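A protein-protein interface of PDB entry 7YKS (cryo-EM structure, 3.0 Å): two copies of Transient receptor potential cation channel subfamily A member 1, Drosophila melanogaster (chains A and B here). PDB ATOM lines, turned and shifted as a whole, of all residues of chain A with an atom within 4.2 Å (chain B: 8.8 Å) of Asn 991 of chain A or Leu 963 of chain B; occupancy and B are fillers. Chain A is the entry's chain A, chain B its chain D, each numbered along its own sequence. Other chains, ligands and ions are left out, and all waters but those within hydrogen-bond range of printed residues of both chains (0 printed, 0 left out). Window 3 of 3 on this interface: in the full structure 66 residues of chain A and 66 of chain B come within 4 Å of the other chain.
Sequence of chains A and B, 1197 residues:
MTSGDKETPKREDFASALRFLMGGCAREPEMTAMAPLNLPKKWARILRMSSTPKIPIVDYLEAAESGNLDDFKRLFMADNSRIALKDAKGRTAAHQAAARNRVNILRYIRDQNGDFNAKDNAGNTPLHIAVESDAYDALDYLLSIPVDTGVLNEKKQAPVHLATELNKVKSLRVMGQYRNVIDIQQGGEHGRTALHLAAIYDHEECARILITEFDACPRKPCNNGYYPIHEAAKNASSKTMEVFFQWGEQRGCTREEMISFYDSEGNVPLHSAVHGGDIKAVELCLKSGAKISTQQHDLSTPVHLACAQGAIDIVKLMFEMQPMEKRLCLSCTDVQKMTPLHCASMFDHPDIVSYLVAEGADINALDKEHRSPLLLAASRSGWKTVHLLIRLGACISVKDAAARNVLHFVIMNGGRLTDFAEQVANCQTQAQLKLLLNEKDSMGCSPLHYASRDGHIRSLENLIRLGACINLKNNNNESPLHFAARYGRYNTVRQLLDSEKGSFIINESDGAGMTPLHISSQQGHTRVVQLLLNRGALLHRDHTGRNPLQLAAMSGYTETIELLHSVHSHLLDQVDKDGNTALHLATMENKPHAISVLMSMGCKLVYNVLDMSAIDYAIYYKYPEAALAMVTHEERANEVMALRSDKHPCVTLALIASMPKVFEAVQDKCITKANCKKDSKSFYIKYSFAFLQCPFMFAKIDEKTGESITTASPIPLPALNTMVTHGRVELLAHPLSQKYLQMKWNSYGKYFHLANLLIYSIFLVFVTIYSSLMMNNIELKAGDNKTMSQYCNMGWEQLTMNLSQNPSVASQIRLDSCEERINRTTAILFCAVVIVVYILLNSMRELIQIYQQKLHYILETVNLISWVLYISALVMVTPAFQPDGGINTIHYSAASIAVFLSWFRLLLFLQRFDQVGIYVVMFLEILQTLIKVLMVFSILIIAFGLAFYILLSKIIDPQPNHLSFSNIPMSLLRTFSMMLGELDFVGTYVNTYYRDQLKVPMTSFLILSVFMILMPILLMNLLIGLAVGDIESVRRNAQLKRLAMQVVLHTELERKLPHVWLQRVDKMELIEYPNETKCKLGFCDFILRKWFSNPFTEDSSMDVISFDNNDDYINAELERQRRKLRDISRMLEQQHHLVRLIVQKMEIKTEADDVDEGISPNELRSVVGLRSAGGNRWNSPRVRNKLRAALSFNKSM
OD1 of Asn 991 of chain A lies close to O of Val 986 of chain A (2.8 Å).
NH1 of Arg 995 of chain A sits close to O of Asn 991 of chain A (3.4 Å).
OG of Ser 966 of chain B is in hydrogen-bond range of O of Leu 963 of chain B, 3.3 Å away.
The backbone carbonyl oxygen (O) of Asn 967 of chain B sits at hydrogen-bond distance from the side-chain hydroxyl (OG) of Ser 971 of chain B (2.6 Å).
The side-chain amide nitrogen (ND2) of Asn 991 of chain A sits close to the backbone carbonyl oxygen (O) of Pro 960 of chain B.
OH of Tyr 994 of chain A sits at hydrogen-bond distance from OG of Ser 966 of chain B (3.3 Å).
OH of Tyr 994 of chain A is in hydrogen-bond range of ND2 of Asn 967 of chain B (3.0 Å).
Of chain B, only Pro 960 and Leu 963 come within 4 Å of Asn 991 of chain A.
Of the printed residues of chain A, Leu 963 of chain B touches Asn 991 (3.8 Å) and Tyr 994 (3.4 Å).
Of the printed residues of chain B, Val 990 of chain A touches Ser 964 (3.8 Å).
Thr 992 of chain A touches none of the printed residues of chain B.
Of the printed residues of chain B, Val 986 of chain A touches Ser 964 (3.96 Å) and Arg 974 (3.4 Å).
Printed residues of chain B within 4 Å of Tyr 994 of chain A: Leu 963 (3.4 Å), Ser 966 (3.3 Å) and Asn 967 (3.0 Å).
Printed residues of chain A within 4 Å of Pro 960 of chain B: Asn 991.
Of the printed residues of chain A, Arg 974 of chain B touches Val 986.
Of the printed residues of chain A, Ser 966 of chain B touches Tyr 994.
Ser 953 of chain B touches none of the printed residues of chain A.
Arg 995 of chain A touches none of the printed residues of chain B.
The nearest residue of chain B that does not touch Asn 991 of chain A is Asn 961 of chain B (5.2 Å).
The nearest printed residue of chain A that does not touch Leu 963 of chain B is Val 990 of chain A (4.3 Å).
Ser 964 of chain B touches Val 986 of chain A.
CG1 of Val 986 of chain A touches NE of Arg 974 of chain B, 3.4 Å away.
Ser 964 of chain B touches Val 990 of chain A (CB to CG1, 3.8 Å).
Leu 963 of chain B touches Asn 991 of chain A (CD2 to ND2, 3.8 Å).
Tyr 994 of chain A touches Leu 963 of chain B (CE2 to O, 3.4 Å).
No position is printed for both chains.
Of the 8 pairs that touch across the chains among the printed residues, none has its exchanged pair printed and touching as well.
Of the 8 printed residues of chain A, 4 touch a printed residue of chain B.
Hydrophobic or aromatic side chains of chain A within 4 Å of the printed part of chain B: Val 986, Val 990 and Tyr 994.
Among the printed residues, no Asp or Glu carboxylate lies within 4 Å of a Lys or Arg side-chain nitrogen of the other chain.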
ATOM      1  N   VAL A 986       7.129  -7.672  23.221  1.00  0.00           N
ATOM      2  CA  VAL A 986       5.792  -7.409  22.718  1.00  0.00           C
ATOM      3  C   VAL A 986       5.371  -5.962  22.948  1.00  0.00           C
ATOM      4  O   VAL A 986       4.189  -5.664  22.931  1.00  0.00           O
ATOM      5  CB  VAL A 986       4.765  -8.377  23.317  1.00  0.00           C
ATOM      6  CG1 VAL A 986       5.045  -9.753  22.845  1.00  0.00           C
ATOM      7  CG2 VAL A 986       4.831  -8.339  24.815  1.00  0.00           C
ATOM      8  N   TYR A 989       8.551  -4.399  19.497  1.00  0.00           N
ATOM      9  CA  TYR A 989       8.679  -5.082  18.220  1.00  0.00           C
ATOM     10  C   TYR A 989       7.360  -5.592  17.678  1.00  0.00           C
ATOM     11  O   TYR A 989       7.125  -5.498  16.478  1.00  0.00           O
ATOM     12  CB  TYR A 989       9.654  -6.260  18.336  1.00  0.00           C
ATOM     13  CG  TYR A 989      11.070  -5.844  18.612  1.00  0.00           C
ATOM     14  CD1 TYR A 989      11.890  -5.383  17.597  1.00  0.00           C
ATOM     15  CD2 TYR A 989      11.587  -5.912  19.892  1.00  0.00           C
ATOM     16  CE1 TYR A 989      13.179  -4.994  17.855  1.00  0.00           C
ATOM     17  CE2 TYR A 989      12.871  -5.516  20.162  1.00  0.00           C
ATOM     18  CZ  TYR A 989      13.664  -5.064  19.141  1.00  0.00           C
ATOM     19  OH  TYR A 989      14.952  -4.680  19.411  1.00  0.00           O
ATOM     20  N   VAL A 990       6.490  -6.132  18.525  1.00  0.00           N
ATOM     21  CA  VAL A 990       5.273  -6.759  18.026  1.00  0.00           C
ATOM     22  C   VAL A 990       4.210  -5.719  17.717  1.00  0.00           C
ATOM     23  O   VAL A 990       3.650  -5.703  16.617  1.00  0.00           O
ATOM     24  CB  VAL A 990       4.764  -7.809  19.024  1.00  0.00           C
ATOM     25  CG1 VAL A 990       3.423  -8.333  18.591  1.00  0.00           C
ATOM     26  CG2 VAL A 990       5.735  -8.933  19.099  1.00  0.00           C
ATOM     27  N   ASN A 991       3.914  -4.830  18.664  1.00  0.00           N
ATOM     28  CA  ASN A 991       2.827  -3.888  18.442  1.00  0.00           C
ATOM     29  C   ASN A 991       3.179  -2.778  17.473  1.00  0.00           C
ATOM     30  O   ASN A 991       2.271  -2.153  16.923  1.00  0.00           O
ATOM     31  CB  ASN A 991       2.350  -3.271  19.750  1.00  0.00           C
ATOM     32  CG  ASN A 991       1.708  -4.278  20.641  1.00  0.00           C
ATOM     33  OD1 ASN A 991       1.983  -4.345  21.830  1.00  0.00           O
ATOM     34  ND2 ASN A 991       0.904  -5.142  20.043  1.00  0.00           N
ATOM     35  N   THR A 992       4.457  -2.518  17.244  1.00  0.00           N
ATOM     36  CA  THR A 992       4.823  -1.566  16.213  1.00  0.00           C
ATOM     37  C   THR A 992       4.911  -2.202  14.841  1.00  0.00           C
ATOM     38  O   THR A 992       4.894  -1.482  13.840  1.00  0.00           O
ATOM     39  CB  THR A 992       6.143  -0.895  16.568  1.00  0.00           C
ATOM     40  OG1 THR A 992       7.162  -1.886  16.682  1.00  0.00           O
ATOM     41  CG2 THR A 992       6.001  -0.197  17.878  1.00  0.00           C
ATOM     42  N   TYR A 993       4.987  -3.527  14.767  1.00  0.00           N
ATOM     43  CA  TYR A 993       4.989  -4.196  13.475  1.00  0.00           C
ATOM     44  C   TYR A 993       3.585  -4.292  12.901  1.00  0.00           C
ATOM     45  O   TYR A 993       3.403  -4.176  11.685  1.00  0.00           O
ATOM     46  CB  TYR A 993       5.613  -5.582  13.609  1.00  0.00           C
ATOM     47  CG  TYR A 993       5.636  -6.382  12.339  1.00  0.00           C
ATOM     48  CD1 TYR A 993       6.498  -6.056  11.310  1.00  0.00           C
ATOM     49  CD2 TYR A 993       4.813  -7.480  12.181  1.00  0.00           C
ATOM     50  CE1 TYR A 993       6.522  -6.789  10.149  1.00  0.00           C
ATOM     51  CE2 TYR A 993       4.830  -8.217  11.025  1.00  0.00           C
ATOM     52  CZ  TYR A 993       5.685  -7.867  10.016  1.00  0.00           C
ATOM     53  OH  TYR A 993       5.704  -8.607   8.863  1.00  0.00           O
ATOM     54  N   TYR A 994       2.586  -4.492  13.754  1.00  0.00           N
ATOM     55  CA  TYR A 994       1.209  -4.598  13.303  1.00  0.00           C
ATOM     56  C   TYR A 994       0.507  -3.253  13.201  1.00  0.00           C
ATOM     57  O   TYR A 994      -0.574  -3.181  12.608  1.00  0.00           O
ATOM     58  CB  TYR A 994       0.421  -5.528  14.223  1.00  0.00           C
ATOM     59  CG  TYR A 994       0.810  -6.975  14.069  1.00  0.00           C
ATOM     60  CD1 TYR A 994       0.374  -7.711  12.981  1.00  0.00           C
ATOM     61  CD2 TYR A 994       1.599  -7.608  15.011  1.00  0.00           C
ATOM     62  CE1 TYR A 994       0.725  -9.029  12.828  1.00  0.00           C
ATOM     63  CE2 TYR A 994       1.955  -8.931  14.867  1.00  0.00           C
ATOM     64  CZ  TYR A 994       1.512  -9.633  13.772  1.00  0.00           C
ATOM     65  OH  TYR A 994       1.857 -10.951  13.618  1.00  0.00           O
ATOM     66  N   ARG A 995       1.080  -2.192  13.754  1.00  0.00           N
ATOM     67  CA  ARG A 995       0.633  -0.845  13.440  1.00  0.00           C
ATOM     68  C   ARG A 995       1.331  -0.276  12.217  1.00  0.00           C
ATOM     69  O   ARG A 995       1.096   0.892  11.886  1.00  0.00           O
ATOM     70  CB  ARG A 995       0.852   0.093  14.628  1.00  0.00           C
ATOM     71  CG  ARG A 995      -0.093  -0.131  15.786  1.00  0.00           C
ATOM     72  CD  ARG A 995      -0.027   1.020  16.771  1.00  0.00           C
ATOM     73  NE  ARG A 995       1.275   1.128  17.421  1.00  0.00           N
ATOM     74  CZ  ARG A 995       1.583   0.542  18.572  1.00  0.00           C
ATOM     75  NH1 ARG A 995       0.680  -0.189  19.211  1.00  0.00           N
ATOM     76  NH2 ARG A 995       2.793   0.693  19.091  1.00  0.00           N
ATOM     77  N   LEU B 952      -4.137 -19.936  21.267  1.00  0.00           N
ATOM     78  CA  LEU B 952      -4.196 -18.517  21.598  1.00  0.00           C
ATOM     79  C   LEU B 952      -4.324 -17.618  20.374  1.00  0.00           C
ATOM     80  O   LEU B 952      -4.055 -16.421  20.474  1.00  0.00           O
ATOM     81  CB  LEU B 952      -2.959 -18.116  22.402  1.00  0.00           C
ATOM     82  CG  LEU B 952      -2.724 -18.746  23.774  1.00  0.00           C
ATOM     83  CD1 LEU B 952      -1.370 -18.351  24.287  1.00  0.00           C
ATOM     84  CD2 LEU B 952      -3.783 -18.329  24.754  1.00  0.00           C
ATOM     85  N   SER B 953      -4.732 -18.146  19.225  1.00  0.00           N
ATOM     86  CA  SER B 953      -4.787 -17.322  18.024  1.00  0.00           C
ATOM     87  C   SER B 953      -6.189 -16.882  17.642  1.00  0.00           C
ATOM     88  O   SER B 953      -6.338 -15.836  17.004  1.00  0.00           O
ATOM     89  CB  SER B 953      -4.162 -18.059  16.839  1.00  0.00           C
ATOM     90  OG  SER B 953      -4.895 -19.221  16.521  1.00  0.00           O
ATOM     91  N   ILE B 955      -8.572 -15.860  19.702  1.00  0.00           N
ATOM     92  CA  ILE B 955      -9.180 -15.116  20.798  1.00  0.00           C
ATOM     93  C   ILE B 955      -9.876 -13.887  20.228  1.00  0.00           C
ATOM     94  O   ILE B 955      -9.267 -13.098  19.498  1.00  0.00           O
ATOM     95  CB  ILE B 955      -8.132 -14.745  21.855  1.00  0.00           C
ATOM     96  CG1 ILE B 955      -7.712 -16.007  22.604  1.00  0.00           C
ATOM     97  CG2 ILE B 955      -8.645 -13.683  22.806  1.00  0.00           C
ATOM     98  CD1 ILE B 955      -6.586 -15.809  23.531  1.00  0.00           C
ATOM     99  N   ASP B 957     -11.485 -10.259  19.902  1.00  0.00           N
ATOM    100  CA  ASP B 957     -10.911  -8.952  20.221  1.00  0.00           C
ATOM    101  C   ASP B 957      -9.450  -9.148  20.607  1.00  0.00           C
ATOM    102  O   ASP B 957      -9.117  -9.091  21.799  1.00  0.00           O
ATOM    103  CB  ASP B 957     -11.692  -8.238  21.333  1.00  0.00           C
ATOM    104  CG  ASP B 957     -11.330  -6.763  21.463  1.00  0.00           C
ATOM    105  OD1 ASP B 957     -10.498  -6.262  20.677  1.00  0.00           O
ATOM    106  OD2 ASP B 957     -11.880  -6.104  22.369  1.00  0.00           O
ATOM    107  N   PRO B 958      -8.554  -9.428  19.636  1.00  0.00           N
ATOM    108  CA  PRO B 958      -7.147  -9.660  19.986  1.00  0.00           C
ATOM    109  C   PRO B 958      -6.448  -8.404  20.480  1.00  0.00           C
ATOM    110  O   PRO B 958      -6.248  -7.433  19.744  1.00  0.00           O
ATOM    111  CB  PRO B 958      -6.538 -10.172  18.676  1.00  0.00           C
ATOM    112  CG  PRO B 958      -7.397  -9.594  17.610  1.00  0.00           C
ATOM    113  CD  PRO B 958      -8.781  -9.521  18.182  1.00  0.00           C
ATOM    114  N   GLN B 959      -6.089  -8.425  21.758  1.00  0.00           N
ATOM    115  CA  GLN B 959      -5.362  -7.341  22.381  1.00  0.00           C
ATOM    116  C   GLN B 959      -3.917  -7.332  21.885  1.00  0.00           C
ATOM    117  O   GLN B 959      -3.470  -8.280  21.238  1.00  0.00           O
ATOM    118  CB  GLN B 959      -5.439  -7.485  23.903  1.00  0.00           C
ATOM    119  CG  GLN B 959      -6.798  -7.136  24.472  1.00  0.00           C
ATOM    120  CD  GLN B 959      -6.842  -7.255  25.979  1.00  0.00           C
ATOM    121  OE1 GLN B 959      -5.890  -7.718  26.607  1.00  0.00           O
ATOM    122  NE2 GLN B 959      -7.946  -6.816  26.575  1.00  0.00           N
ATOM    123  N   PRO B 960      -3.155  -6.247  22.160  1.00  0.00           N
ATOM    124  CA  PRO B 960      -1.696  -6.277  21.951  1.00  0.00           C
ATOM    125  C   PRO B 960      -0.924  -7.410  22.620  1.00  0.00           C
ATOM    126  O   PRO B 960       0.198  -7.715  22.206  1.00  0.00           O
ATOM    127  CB  PRO B 960      -1.263  -4.920  22.515  1.00  0.00           C
ATOM    128  CG  PRO B 960      -2.389  -4.038  22.179  1.00  0.00           C
ATOM    129  CD  PRO B 960      -3.633  -4.862  22.349  1.00  0.00           C
ATOM    130  N   ASN B 961      -1.503  -8.030  23.650  1.00  0.00           N
ATOM    131  CA  ASN B 961      -0.899  -9.202  24.273  1.00  0.00           C
ATOM    132  C   ASN B 961      -0.900 -10.397  23.327  1.00  0.00           C
ATOM    133  O   ASN B 961       0.150 -10.991  23.056  1.00  0.00           O
ATOM    134  CB  ASN B 961      -1.653  -9.539  25.556  1.00  0.00           C
ATOM    135  CG  ASN B 961      -1.551  -8.449  26.593  1.00  0.00           C
ATOM    136  OD1 ASN B 961      -2.546  -7.822  26.952  1.00  0.00           O
ATOM    137  ND2 ASN B 961      -0.341  -8.215  27.088  1.00  0.00           N
ATOM    138  N   HIS B 962      -2.073 -10.763  22.811  1.00  0.00           N
ATOM    139  CA  HIS B 962      -2.246 -11.966  22.008  1.00  0.00           C
ATOM    140  C   HIS B 962      -2.050 -11.729  20.528  1.00  0.00           C
ATOM    141  O   HIS B 962      -2.412 -12.588  19.722  1.00  0.00           O
ATOM    142  CB  HIS B 962      -3.631 -12.556  22.230  1.00  0.00           C
ATOM    143  CG  HIS B 962      -3.851 -13.049  23.617  1.00  0.00           C
ATOM    144  ND1 HIS B 962      -4.405 -12.265  24.602  1.00  0.00           N
ATOM    145  CD2 HIS B 962      -3.552 -14.232  24.196  1.00  0.00           C
ATOM    146  CE1 HIS B 962      -4.459 -12.956  25.725  1.00  0.00           C
ATOM    147  NE2 HIS B 962      -3.954 -14.154  25.504  1.00  0.00           N
ATOM    148  N   LEU B 963      -1.495 -10.591  20.150  1.00  0.00           N
ATOM    149  CA  LEU B 963      -1.274 -10.306  18.747  1.00  0.00           C
ATOM    150  C   LEU B 963       0.013 -10.936  18.247  1.00  0.00           C
ATOM    151  O   LEU B 963       0.274 -10.923  17.043  1.00  0.00           O
ATOM    152  CB  LEU B 963      -1.272  -8.789  18.556  1.00  0.00           C
ATOM    153  CG  LEU B 963      -1.484  -8.151  17.195  1.00  0.00           C
ATOM    154  CD1 LEU B 963      -2.858  -8.519  16.693  1.00  0.00           C
ATOM    155  CD2 LEU B 963      -1.364  -6.658  17.346  1.00  0.00           C
ATOM    156  N   SER B 964       0.808 -11.508  19.145  1.00  0.00           N
ATOM    157  CA  SER B 964       2.055 -12.170  18.805  1.00  0.00           C
ATOM    158  C   SER B 964       1.906 -13.668  18.619  1.00  0.00           C
ATOM    159  O   SER B 964       2.903 -14.341  18.362  1.00  0.00           O
ATOM    160  CB  SER B 964       3.101 -11.896  19.882  1.00  0.00           C
ATOM    161  OG  SER B 964       2.695 -12.434  21.118  1.00  0.00           O
ATOM    162  N   PHE B 965       0.698 -14.211  18.755  1.00  0.00           N
ATOM    163  CA  PHE B 965       0.440 -15.613  18.461  1.00  0.00           C
ATOM    164  C   PHE B 965      -0.468 -15.787  17.256  1.00  0.00           C
ATOM    165  O   PHE B 965      -1.140 -16.809  17.143  1.00  0.00           O
ATOM    166  CB  PHE B 965      -0.177 -16.329  19.661  1.00  0.00           C
ATOM    167  CG  PHE B 965       0.736 -16.449  20.835  1.00  0.00           C
ATOM    168  CD1 PHE B 965       1.810 -17.319  20.809  1.00  0.00           C
ATOM    169  CD2 PHE B 965       0.488 -15.737  21.988  1.00  0.00           C
ATOM    170  CE1 PHE B 965       2.644 -17.439  21.894  1.00  0.00           C
ATOM    171  CE2 PHE B 965       1.317 -15.859  23.075  1.00  0.00           C
ATOM    172  CZ  PHE B 965       2.392 -16.712  23.028  1.00  0.00           C
ATOM    173  N   SER B 966      -0.509 -14.811  16.357  1.00  0.00           N
ATOM    174  CA  SER B 966      -1.392 -14.884  15.204  1.00  0.00           C
ATOM    175  C   SER B 966      -0.722 -15.468  13.970  1.00  0.00           C
ATOM    176  O   SER B 966      -1.399 -15.674  12.960  1.00  0.00           O
ATOM    177  CB  SER B 966      -1.944 -13.496  14.880  1.00  0.00           C
ATOM    178  OG  SER B 966      -0.907 -12.622  14.487  1.00  0.00           O
ATOM    179  N   ASN B 967       0.576 -15.736  14.023  1.00  0.00           N
ATOM    180  CA  ASN B 967       1.305 -16.406  12.959  1.00  0.00           C
ATOM    181  C   ASN B 967       2.062 -17.588  13.540  1.00  0.00           C
ATOM    182  O   ASN B 967       2.215 -17.721  14.751  1.00  0.00           O
ATOM    183  CB  ASN B 967       2.297 -15.465  12.279  1.00  0.00           C
ATOM    184  CG  ASN B 967       1.624 -14.364  11.532  1.00  0.00           C
ATOM    185  OD1 ASN B 967       0.614 -14.581  10.868  1.00  0.00           O
ATOM    186  ND2 ASN B 967       2.172 -13.163  11.634  1.00  0.00           N
ATOM    187  N   MET B 970       5.703 -15.904  14.036  1.00  0.00           N
ATOM    188  CA  MET B 970       5.718 -14.980  15.161  1.00  0.00           C
ATOM    189  C   MET B 970       5.539 -15.716  16.482  1.00  0.00           C
ATOM    190  O   MET B 970       6.002 -15.240  17.521  1.00  0.00           O
ATOM    191  CB  MET B 970       4.636 -13.918  14.961  1.00  0.00           C
ATOM    192  CG  MET B 970       4.643 -12.771  15.955  1.00  0.00           C
ATOM    193  SD  MET B 970       6.118 -11.749  15.897  1.00  0.00           S
ATOM    194  CE  MET B 970       5.817 -10.837  14.397  1.00  0.00           C
ATOM    195  N   SER B 971       4.906 -16.888  16.458  1.00  0.00           N
ATOM    196  CA  SER B 971       4.786 -17.696  17.662  1.00  0.00           C
ATOM    197  C   SER B 971       6.086 -18.391  18.022  1.00  0.00           C
ATOM    198  O   SER B 971       6.250 -18.804  19.172  1.00  0.00           O
ATOM    199  CB  SER B 971       3.692 -18.741  17.492  1.00  0.00           C
ATOM    200  OG  SER B 971       2.442 -18.123  17.300  1.00  0.00           O
ATOM    201  N   ARG B 974       8.088 -15.607  19.832  1.00  0.00           N
ATOM    202  CA  ARG B 974       7.511 -15.305  21.132  1.00  0.00           C
ATOM    203  C   ARG B 974       7.855 -16.387  22.140  1.00  0.00           C
ATOM    204  O   ARG B 974       8.174 -16.085  23.292  1.00  0.00           O
ATOM    205  CB  ARG B 974       6.004 -15.156  21.009  1.00  0.00           C
ATOM    206  CG  ARG B 974       5.333 -14.782  22.291  1.00  0.00           C
ATOM    207  CD  ARG B 974       5.591 -13.347  22.621  1.00  0.00           C
ATOM    208  NE  ARG B 974       4.983 -12.969  23.888  1.00  0.00           N
ATOM    209  CZ  ARG B 974       5.629 -12.921  25.044  1.00  0.00           C
ATOM    210  NH1 ARG B 974       4.985 -12.576  26.142  1.00  0.00           N
ATOM    211  NH2 ARG B 974       6.924 -13.175  25.097  1.00  0.00           N
ATOM    212  N   THR B 988      -1.898 -12.216  29.781  1.00  0.00           N
ATOM    213  CA  THR B 988      -2.323 -13.031  28.658  1.00  0.00           C
ATOM    214  C   THR B 988      -3.133 -14.247  29.073  1.00  0.00           C
ATOM    215  O   THR B 988      -3.782 -14.853  28.217  1.00  0.00           O
ATOM    216  CB  THR B 988      -1.108 -13.498  27.845  1.00  0.00           C
ATOM    217  OG1 THR B 988      -0.291 -14.333  28.654  1.00  0.00           O
ATOM    218  CG2 THR B 988      -0.265 -12.335  27.444  1.00  0.00           C
